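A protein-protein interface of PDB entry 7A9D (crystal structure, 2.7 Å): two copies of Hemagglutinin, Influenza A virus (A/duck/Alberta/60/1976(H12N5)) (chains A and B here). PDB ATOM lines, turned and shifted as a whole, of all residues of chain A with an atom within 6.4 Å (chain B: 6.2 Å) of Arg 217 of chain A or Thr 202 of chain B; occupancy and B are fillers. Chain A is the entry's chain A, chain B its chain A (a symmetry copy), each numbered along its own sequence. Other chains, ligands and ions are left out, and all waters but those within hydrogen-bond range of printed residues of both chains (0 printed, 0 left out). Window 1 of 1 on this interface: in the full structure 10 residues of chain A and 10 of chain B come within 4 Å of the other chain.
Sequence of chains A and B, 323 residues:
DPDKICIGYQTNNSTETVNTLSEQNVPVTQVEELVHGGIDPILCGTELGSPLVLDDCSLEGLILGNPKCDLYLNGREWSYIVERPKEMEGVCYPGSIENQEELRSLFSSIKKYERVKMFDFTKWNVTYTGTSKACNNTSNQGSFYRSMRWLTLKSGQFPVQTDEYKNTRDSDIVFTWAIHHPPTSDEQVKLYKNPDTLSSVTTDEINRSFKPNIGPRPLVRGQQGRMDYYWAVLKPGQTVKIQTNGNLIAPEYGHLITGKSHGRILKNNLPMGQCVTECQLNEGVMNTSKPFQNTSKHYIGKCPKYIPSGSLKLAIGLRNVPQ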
ATOM      1  N   HIS A 181       8.397   7.273 -36.221  1.00  0.00           N
ATOM      2  CA  HIS A 181       8.858   8.445 -35.429  1.00  0.00           C
ATOM      3  C   HIS A 181      10.156   8.082 -34.709  1.00  0.00           C
ATOM      4  O   HIS A 181      10.118   7.509 -33.621  1.00  0.00           O
ATOM      5  CB  HIS A 181       7.762   8.892 -34.451  1.00  0.00           C
ATOM      6  CG  HIS A 181       6.476   9.258 -35.111  1.00  0.00           C
ATOM      7  ND1 HIS A 181       6.227  10.529 -35.587  1.00  0.00           N
ATOM      8  CD2 HIS A 181       5.372   8.528 -35.378  1.00  0.00           C
ATOM      9  CE1 HIS A 181       5.022  10.569 -36.117  1.00  0.00           C
ATOM     10  NE2 HIS A 181       4.476   9.352 -36.003  1.00  0.00           N
ATOM     11  N   PRO A 182      11.340   8.379 -35.297  1.00  0.00           N
ATOM     12  CA  PRO A 182      12.618   8.056 -34.661  1.00  0.00           C
ATOM     13  C   PRO A 182      12.763   8.645 -33.260  1.00  0.00           C
ATOM     14  O   PRO A 182      12.200   9.698 -32.967  1.00  0.00           O
ATOM     15  CB  PRO A 182      13.661   8.683 -35.599  1.00  0.00           C
ATOM     16  CG  PRO A 182      12.970   8.728 -36.942  1.00  0.00           C
ATOM     17  CD  PRO A 182      11.517   9.011 -36.614  1.00  0.00           C
ATOM     18  N   PRO A 183      13.524   7.986 -32.356  1.00  0.00           N
ATOM     19  CA  PRO A 183      13.732   8.503 -31.002  1.00  0.00           C
ATOM     20  C   PRO A 183      14.695   9.703 -30.966  1.00  0.00           C
ATOM     21  O   PRO A 183      14.343  10.710 -30.376  1.00  0.00           O
ATOM     22  CB  PRO A 183      14.306   7.295 -30.242  1.00  0.00           C
ATOM     23  CG  PRO A 183      14.988   6.456 -31.308  1.00  0.00           C
ATOM     24  CD  PRO A 183      14.218   6.709 -32.588  1.00  0.00           C
ATOM     25  N   ASN A 213       8.138  13.570 -35.885  1.00  0.00           N
ATOM     26  CA  ASN A 213       8.537  14.446 -34.750  1.00  0.00           C
ATOM     27  C   ASN A 213       9.533  13.684 -33.868  1.00  0.00           C
ATOM     28  O   ASN A 213       9.109  12.748 -33.161  1.00  0.00           O
ATOM     29  CB  ASN A 213       7.321  14.970 -33.979  1.00  0.00           C
ATOM     30  CG  ASN A 213       6.115  14.058 -34.072  1.00  0.00           C
ATOM     31  OD1 ASN A 213       5.041  14.485 -34.488  1.00  0.00           O
ATOM     32  ND2 ASN A 213       6.284  12.803 -33.695  1.00  0.00           N
ATOM     33  N   ILE A 214      10.809  14.079 -33.925  1.00  0.00           N
ATOM     34  CA  ILE A 214      11.952  13.384 -33.261  1.00  0.00           C
ATOM     35  C   ILE A 214      11.829  13.600 -31.749  1.00  0.00           C
ATOM     36  O   ILE A 214      11.775  14.770 -31.319  1.00  0.00           O
ATOM     37  CB  ILE A 214      13.305  13.872 -33.823  1.00  0.00           C
ATOM     38  CG1 ILE A 214      13.547  13.361 -35.248  1.00  0.00           C
ATOM     39  CG2 ILE A 214      14.456  13.496 -32.897  1.00  0.00           C
ATOM     40  CD1 ILE A 214      12.858  14.165 -36.330  1.00  0.00           C
ATOM     41  N   GLY A 215      11.777  12.504 -30.986  1.00  0.00           N
ATOM     42  CA  GLY A 215      11.637  12.505 -29.516  1.00  0.00           C
ATOM     43  C   GLY A 215      11.552  11.081 -28.974  1.00  0.00           C
ATOM     44  O   GLY A 215      10.729  10.301 -29.446  1.00  0.00           O
ATOM     45  N   PRO A 216      12.388  10.688 -27.984  1.00  0.00           N
ATOM     46  CA  PRO A 216      12.391   9.309 -27.495  1.00  0.00           C
ATOM     47  C   PRO A 216      11.094   8.965 -26.742  1.00  0.00           C
ATOM     48  O   PRO A 216      10.479   9.864 -26.190  1.00  0.00           O
ATOM     49  CB  PRO A 216      13.609   9.195 -26.562  1.00  0.00           C
ATOM     50  CG  PRO A 216      14.282  10.563 -26.567  1.00  0.00           C
ATOM     51  CD  PRO A 216      13.360  11.533 -27.279  1.00  0.00           C
ATOM     52  N   ARG A 217      10.718   7.683 -26.752  1.00  0.00           N
ATOM     53  CA  ARG A 217       9.522   7.132 -26.058  1.00  0.00           C
ATOM     54  C   ARG A 217       9.974   6.099 -25.029  1.00  0.00           C
ATOM     55  O   ARG A 217      11.104   5.621 -25.086  1.00  0.00           O
ATOM     56  CB  ARG A 217       8.561   6.494 -27.069  1.00  0.00           C
ATOM     57  CG  ARG A 217       7.663   7.482 -27.802  1.00  0.00           C
ATOM     58  CD  ARG A 217       8.296   8.074 -29.047  1.00  0.00           C
ATOM     59  NE  ARG A 217       7.439   9.081 -29.661  1.00  0.00           N
ATOM     60  CZ  ARG A 217       7.771   9.838 -30.706  1.00  0.00           C
ATOM     61  NH1 ARG A 217       8.959   9.716 -31.276  1.00  0.00           N
ATOM     62  NH2 ARG A 217       6.908  10.721 -31.177  1.00  0.00           N
ATOM     63  N   PRO A 218       9.116   5.734 -24.048  1.00  0.00           N
ATOM     64  CA  PRO A 218       9.378   4.579 -23.186  1.00  0.00           C
ATOM     65  C   PRO A 218       9.470   3.273 -23.994  1.00  0.00           C
ATOM     66  O   PRO A 218       8.740   3.143 -24.961  1.00  0.00           O
ATOM     67  CB  PRO A 218       8.167   4.532 -22.240  1.00  0.00           C
ATOM     68  CG  PRO A 218       7.582   5.930 -22.292  1.00  0.00           C
ATOM     69  CD  PRO A 218       7.872   6.431 -23.690  1.00  0.00           C
ATOM     70  N   LEU A 219      10.353   2.353 -23.586  1.00  0.00           N
ATOM     71  CA  LEU A 219      10.560   1.036 -24.253  1.00  0.00           C
ATOM     72  C   LEU A 219       9.277   0.204 -24.149  1.00  0.00           C
ATOM     73  O   LEU A 219       8.708   0.135 -23.042  1.00  0.00           O
ATOM     74  CB  LEU A 219      11.738   0.297 -23.603  1.00  0.00           C
ATOM     75  CG  LEU A 219      13.128   0.894 -23.830  1.00  0.00           C
ATOM     76  CD1 LEU A 219      14.200  -0.021 -23.258  1.00  0.00           C
ATOM     77  CD2 LEU A 219      13.393   1.152 -25.306  1.00  0.00           C
ATOM     78  N   GLN A 223      12.401  -1.229 -27.978  1.00  0.00           N
ATOM     79  CA  GLN A 223      12.495  -0.227 -29.073  1.00  0.00           C
ATOM     80  C   GLN A 223      12.115   1.152 -28.520  1.00  0.00           C
ATOM     81  O   GLN A 223      10.991   1.292 -27.997  1.00  0.00           O
ATOM     82  CB  GLN A 223      11.597  -0.634 -30.245  1.00  0.00           C
ATOM     83  CG  GLN A 223      12.221  -0.376 -31.610  1.00  0.00           C
ATOM     84  CD  GLN A 223      13.291  -1.381 -31.969  1.00  0.00           C
ATOM     85  OE1 GLN A 223      13.647  -2.255 -31.181  1.00  0.00           O
ATOM     86  NE2 GLN A 223      13.815  -1.262 -33.178  1.00  0.00           N
ATOM     87  N   GLN A 224      13.030   2.122 -28.632  1.00  0.00           N
ATOM     88  CA  GLN A 224      12.847   3.525 -28.170  1.00  0.00           C
ATOM     89  C   GLN A 224      11.915   4.260 -29.143  1.00  0.00           C
ATOM     90  O   GLN A 224      11.323   5.274 -28.730  1.00  0.00           O
ATOM     91  CB  GLN A 224      14.202   4.232 -28.067  1.00  0.00           C
ATOM     92  CG  GLN A 224      14.227   5.371 -27.057  1.00  0.00           C
ATOM     93  CD  GLN A 224      14.631   4.909 -25.678  1.00  0.00           C
ATOM     94  OE1 GLN A 224      15.749   4.450 -25.459  1.00  0.00           O
ATOM     95  NE2 GLN A 224      13.719   5.039 -24.728  1.00  0.00           N
ATOM     96  N   GLY A 225      11.806   3.769 -30.384  1.00  0.00           N
ATOM     97  CA  GLY A 225      10.960   4.345 -31.449  1.00  0.00           C
ATOM     98  C   GLY A 225       9.497   3.954 -31.304  1.00  0.00           C
ATOM     99  O   GLY A 225       9.165   3.231 -30.341  1.00  0.00           O
ATOM    100  N   ARG A 226       8.654   4.416 -32.233  1.00  0.00           N
ATOM    101  CA  ARG A 226       7.177   4.224 -32.219  1.00  0.00           C
ATOM    102  C   ARG A 226       6.616   4.522 -33.615  1.00  0.00           C
ATOM    103  O   ARG A 226       7.161   5.420 -34.287  1.00  0.00           O
ATOM    104  CB  ARG A 226       6.543   5.134 -31.160  1.00  0.00           C
ATOM    105  CG  ARG A 226       5.092   4.813 -30.835  1.00  0.00           C
ATOM    106  CD  ARG A 226       4.926   3.601 -29.937  1.00  0.00           C
ATOM    107  NE  ARG A 226       4.935   3.940 -28.518  1.00  0.00           N
ATOM    108  CZ  ARG A 226       5.974   3.814 -27.691  1.00  0.00           C
ATOM    109  NH1 ARG A 226       5.842   4.159 -26.421  1.00  0.00           N
ATOM    110  NH2 ARG A 226       7.137   3.346 -28.117  1.00  0.00           N
ATOM    111  N   GLU B 164      10.791  11.904 -16.941  1.00  0.00           N
ATOM    112  CA  GLU B 164      10.007  10.641 -16.942  1.00  0.00           C
ATOM    113  C   GLU B 164       9.290  10.487 -15.594  1.00  0.00           C
ATOM    114  O   GLU B 164       9.840  10.954 -14.579  1.00  0.00           O
ATOM    115  CB  GLU B 164      10.962   9.473 -17.199  1.00  0.00           C
ATOM    116  CG  GLU B 164      10.287   8.209 -17.695  1.00  0.00           C
ATOM    117  CD  GLU B 164      11.245   7.065 -17.991  1.00  0.00           C
ATOM    118  OE1 GLU B 164      12.187   6.862 -17.195  1.00  0.00           O
ATOM    119  OE2 GLU B 164      11.052   6.382 -19.018  1.00  0.00           O
ATOM    120  N   SER B 200       5.548  17.314 -27.001  1.00  0.00           N
ATOM    121  CA  SER B 200       4.999  15.940 -27.166  1.00  0.00           C
ATOM    122  C   SER B 200       4.861  15.231 -25.811  1.00  0.00           C
ATOM    123  O   SER B 200       5.720  15.443 -24.930  1.00  0.00           O
ATOM    124  CB  SER B 200       5.838  15.139 -28.132  1.00  0.00           C
ATOM    125  OG  SER B 200       7.206  15.148 -27.752  1.00  0.00           O
ATOM    126  N   VAL B 201       3.801  14.425 -25.674  1.00  0.00           N
ATOM    127  CA  VAL B 201       3.471  13.592 -24.477  1.00  0.00           C
ATOM    128  C   VAL B 201       3.281  12.151 -24.960  1.00  0.00           C
ATOM    129  O   VAL B 201       2.389  11.935 -25.805  1.00  0.00           O
ATOM    130  CB  VAL B 201       2.211  14.115 -23.758  1.00  0.00           C
ATOM    131  CG1 VAL B 201       2.033  13.476 -22.387  1.00  0.00           C
ATOM    132  CG2 VAL B 201       2.204  15.632 -23.645  1.00  0.00           C
ATOM    133  N   THR B 202       4.088  11.212 -24.454  1.00  0.00           N
ATOM    134  CA  THR B 202       4.151   9.802 -24.931  1.00  0.00           C
ATOM    135  C   THR B 202       4.083   8.837 -23.740  1.00  0.00           C
ATOM    136  O   THR B 202       4.696   9.139 -22.697  1.00  0.00           O
ATOM    137  CB  THR B 202       5.418   9.555 -25.758  1.00  0.00           C
ATOM    138  OG1 THR B 202       6.549   9.634 -24.888  1.00  0.00           O
ATOM    139  CG2 THR B 202       5.585  10.538 -26.896  1.00  0.00           C
ATOM    140  N   THR B 203       3.364   7.721 -23.908  1.00  0.00           N
ATOM    141  CA  THR B 203       3.306   6.577 -22.956  1.00  0.00           C
ATOM    142  C   THR B 203       3.564   5.278 -23.732  1.00  0.00           C
ATOM    143  O   THR B 203       4.012   5.363 -24.896  1.00  0.00           O
ATOM    144  CB  THR B 203       1.973   6.541 -22.192  1.00  0.00           C
ATOM    145  OG1 THR B 203       0.955   6.044 -23.061  1.00  0.00           O
ATOM    146  CG2 THR B 203       1.565   7.891 -21.643  1.00  0.00           C
ATOM    147  N   ASP B 204       3.282   4.128 -23.113  1.00  0.00           N
ATOM    148  CA  ASP B 204       3.480   2.774 -23.700  1.00  0.00           C
ATOM    149  C   ASP B 204       2.403   2.494 -24.759  1.00  0.00           C
ATOM    150  O   ASP B 204       2.613   1.558 -25.559  1.00  0.00           O
ATOM    151  CB  ASP B 204       3.476   1.697 -22.608  1.00  0.00           C
ATOM    152  CG  ASP B 204       4.514   1.908 -21.517  1.00  0.00           C
ATOM    153  OD1 ASP B 204       4.541   1.097 -20.570  1.00  0.00           O
ATOM    154  OD2 ASP B 204       5.286   2.882 -21.618  1.00  0.00           O
ATOM    155  N   ILE B 206       0.033   5.486 -26.100  1.00  0.00           N
ATOM    156  CA  ILE B 206      -0.251   6.732 -26.881  1.00  0.00           C
ATOM    157  C   ILE B 206       1.064   7.397 -27.317  1.00  0.00           C
ATOM    158  O   ILE B 206       2.090   7.210 -26.631  1.00  0.00           O
ATOM    159  CB  ILE B 206      -1.153   7.709 -26.094  1.00  0.00           C
ATOM    160  CG1 ILE B 206      -0.491   8.232 -24.815  1.00  0.00           C
ATOM    161  CG2 ILE B 206      -2.505   7.075 -25.803  1.00  0.00           C
ATOM    162  CD1 ILE B 206      -0.958   9.609 -24.408  1.00  0.00           C
ATOM    163  N   ASN B 207       1.009   8.152 -28.423  1.00  0.00           N
ATOM    164  CA  ASN B 207       2.145   8.910 -29.016  1.00  0.00           C
ATOM    165  C   ASN B 207       1.599  10.200 -29.643  1.00  0.00           C
ATOM    166  O   ASN B 207       1.100  10.136 -30.783  1.00  0.00           O
ATOM    167  CB  ASN B 207       2.907   8.068 -30.044  1.00  0.00           C
ATOM    168  CG  ASN B 207       3.996   8.841 -30.757  1.00  0.00           C
ATOM    169  OD1 ASN B 207       4.685   9.654 -30.149  1.00  0.00           O
ATOM    170  ND2 ASN B 207       4.155   8.595 -32.048  1.00  0.00           N
ATOM    171  N   ARG B 208       1.697  11.319 -28.918  1.00  0.00           N
ATOM    172  CA  ARG B 208       1.039  12.612 -29.252  1.00  0.00           C
ATOM    173  C   ARG B 208       2.091  13.726 -29.300  1.00  0.00           C
ATOM    174  O   ARG B 208       2.927  13.785 -28.379  1.00  0.00           O
ATOM    175  CB  ARG B 208      -0.044  12.917 -28.213  1.00  0.00           C
ATOM    176  CG  ARG B 208      -1.162  11.884 -28.152  1.00  0.00           C
ATOM    177  CD  ARG B 208      -2.473  12.388 -28.722  1.00  0.00           C
ATOM    178  NE  ARG B 208      -3.252  13.126 -27.735  1.00  0.00           N
ATOM    179  CZ  ARG B 208      -4.394  13.763 -27.983  1.00  0.00           C
ATOM    180  NH1 ARG B 208      -4.912  13.770 -29.201  1.00  0.00           N
ATOM    181  NH2 ARG B 208      -5.018  14.400 -27.007  1.00  0.00           N
ATOM    182  N   SER B 209       2.038  14.569 -30.339  1.00  0.00           N
ATOM    183  CA  SER B 209       2.927  15.742 -30.565  1.00  0.00           C
ATOM    184  C   SER B 209       2.080  16.963 -30.943  1.00  0.00           C
ATOM    185  O   SER B 209       1.007  16.768 -31.548  1.00  0.00           O
ATOM    186  CB  SER B 209       3.958  15.442 -31.620  1.00  0.00           C
ATOM    187  OG  SER B 209       4.859  14.442 -31.171  1.00  0.00           O
ATOM    188  N   THR B 239       4.612   4.006 -18.041  1.00  0.00           N
ATOM    189  CA  THR B 239       5.529   5.169 -17.902  1.00  0.00           C
ATOM    190  C   THR B 239       5.079   6.285 -18.853  1.00  0.00           C
ATOM    191  O   THR B 239       4.894   5.994 -20.050  1.00  0.00           O
ATOM    192  CB  THR B 239       6.978   4.751 -18.180  1.00  0.00           C
ATOM    193  OG1 THR B 239       7.298   3.660 -17.316  1.00  0.00           O
ATOM    194  CG2 THR B 239       7.973   5.871 -17.968  1.00  0.00           C
ATOM    195  N   VAL B 240       4.907   7.503 -18.328  1.00  0.00           N
ATOM    196  CA  VAL B 240       4.663   8.750 -19.116  1.00  0.00           C
ATOM    197  C   VAL B 240       5.965   9.560 -19.128  1.00  0.00           C
ATOM    198  O   VAL B 240       6.635   9.619 -18.078  1.00  0.00           O
ATOM    199  CB  VAL B 240       3.481   9.574 -18.563  1.00  0.00           C
ATOM    200  CG1 VAL B 240       3.732  10.100 -17.157  1.00  0.00           C
ATOM    201  CG2 VAL B 240       3.114  10.720 -19.494  1.00  0.00           C
ATOM    202  N   LYS B 241       6.307  10.150 -20.277  1.00  0.00           N
ATOM    203  CA  LYS B 241       7.534  10.967 -20.457  1.00  0.00           C
ATOM    204  C   LYS B 241       7.185  12.234 -21.245  1.00  0.00           C
ATOM    205  O   LYS B 241       6.617  12.109 -22.348  1.00  0.00           O
ATOM    206  CB  LYS B 241       8.619  10.149 -21.159  1.00  0.00           C
ATOM    207  CG  LYS B 241      10.043  10.591 -20.852  1.00  0.00           C
ATOM    208  CD  LYS B 241      11.045  10.207 -21.913  1.00  0.00           C
ATOM    209  CE  LYS B 241      10.987  11.117 -23.122  1.00  0.00           C
ATOM    210  NZ  LYS B 241      11.979  10.723 -24.145  1.00  0.00           N
ATOM    211  N   ILE B 242       7.521  13.401 -20.686  1.00  0.00           N
ATOM    212  CA  ILE B 242       7.255  14.748 -21.275  1.00  0.00           C
ATOM    213  C   ILE B 242       8.529  15.232 -21.982  1.00  0.00           C
ATOM    214  O   ILE B 242       9.629  14.831 -21.553  1.00  0.00           O
ATOM    215  CB  ILE B 242       6.770  15.718 -20.176  1.00  0.00           C
ATOM    216  CG1 ILE B 242       5.827  16.785 -20.732  1.00  0.00           C
ATOM    217  CG2 ILE B 242       7.934  16.330 -19.410  1.00  0.00           C
ATOM    218  CD1 ILE B 242       4.404  16.307 -20.907  1.00  0.00           C
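The guanidinium group (NH2) of Arg 217 of chain A sits at hydrogen-bond distance from the side-chain amide oxygen (OD1) of Asn 207 of chain B (2.7 Å).
The backbone carbonyl oxygen (O) of Pro 216 of chain A sits at hydrogen-bond distance from the side-chain amino group (NZ) of Lys 241 of chain B.
The guanidinium group of Arg 226 of chain A lies within hydrogen-bond range of the backbone carbonyl oxygen of Thr 203 of chain B, at 2.7 Å.
OG of Ser 209 of chain B lies close to OD1 of Asn 213 of chain A.
O of His 181 of chain A lies within hydrogen-bond range of NH1 of Arg 217 of chain A.
NH1 of Arg 226 of chain A lies within hydrogen-bond range of O of Pro 218 of chain A (3.4 Å).
O of Arg 217 of chain A lies within hydrogen-bond range of NE2 of Gln 224 of chain A (2.7 Å).
NH2 of Arg 217 of chain A sits close to ND2 of Asn 213 of chain A, at 3.3 Å.
The backbone carbonyl oxygen (O) of Gly 215 of chain A is in hydrogen-bond range of the guanidinium group (NH1) of Arg 217 of chain A, 2.6 Å away.
A ring nitrogen (ND1) of His 181 of chain A lies within hydrogen-bond range of the side-chain amide nitrogen (ND2) of Asn 213 of chain A (3.0 Å).
His 181 of chain A touches Asn 207 of chain B (CD2 to ND2, 3.5 Å).
Arg 217 of chain A touches Thr 202 of chain B (NE to CG2, 3.6 Å).
Pro 218 of chain A touches Thr 202 of chain B (CD to OG1, 3.7 Å).
CB of Pro 218 of chain A touches OD2 of Asp 204 of chain B, 3.4 Å away.
Pro 218 of chain A touches Thr 239 of chain B (CG to O, 3.5 Å).
Asp 204 of chain B touches Arg 226 of chain A (CA to NH1, 3.9 Å).
Asn 207 of chain B touches Arg 226 of chain A (CB to CG, 3.999 Å).
Of the printed residues of chain B, Arg 217 of chain A touches Thr 202 (3.6 Å) and Asn 207 (2.7 Å).
Of the printed residues of chain B, Pro 218 of chain A touches Thr 202, Asp 204 and Thr 239.
Printed residues of chain B within 4 Å of Arg 226 of chain A: Thr 203 (2.7 Å), Asp 204 (3.9 Å) and Asn 207 (3.999 Å).
Thr 202 of chain B touches just these residues of chain A: Arg 217 and Pro 218.
The nearest residue of chain A that does not touch Thr 202 of chain B is Pro 216 of chain A (4.1 Å).
Along chain B the printed residues that touch a printed residue of chain A span positions 202 to 241.
Of the 14 printed residues of chain A, 6 touch a printed residue of chain B.
Hydrophobic or aromatic side chains of chain A that line the printed part of chain B: His 181, Pro 216 and Pro 218.
Among the printed residues, no Asp or Glu carboxylate lies within 4 Å of a Lys or Arg side-chain nitrogen of the other chain.
No position is printed for both chains.
Of the 11 pairs that touch across the chains among the printed residues, none has its exchanged pair printed and touching as well.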
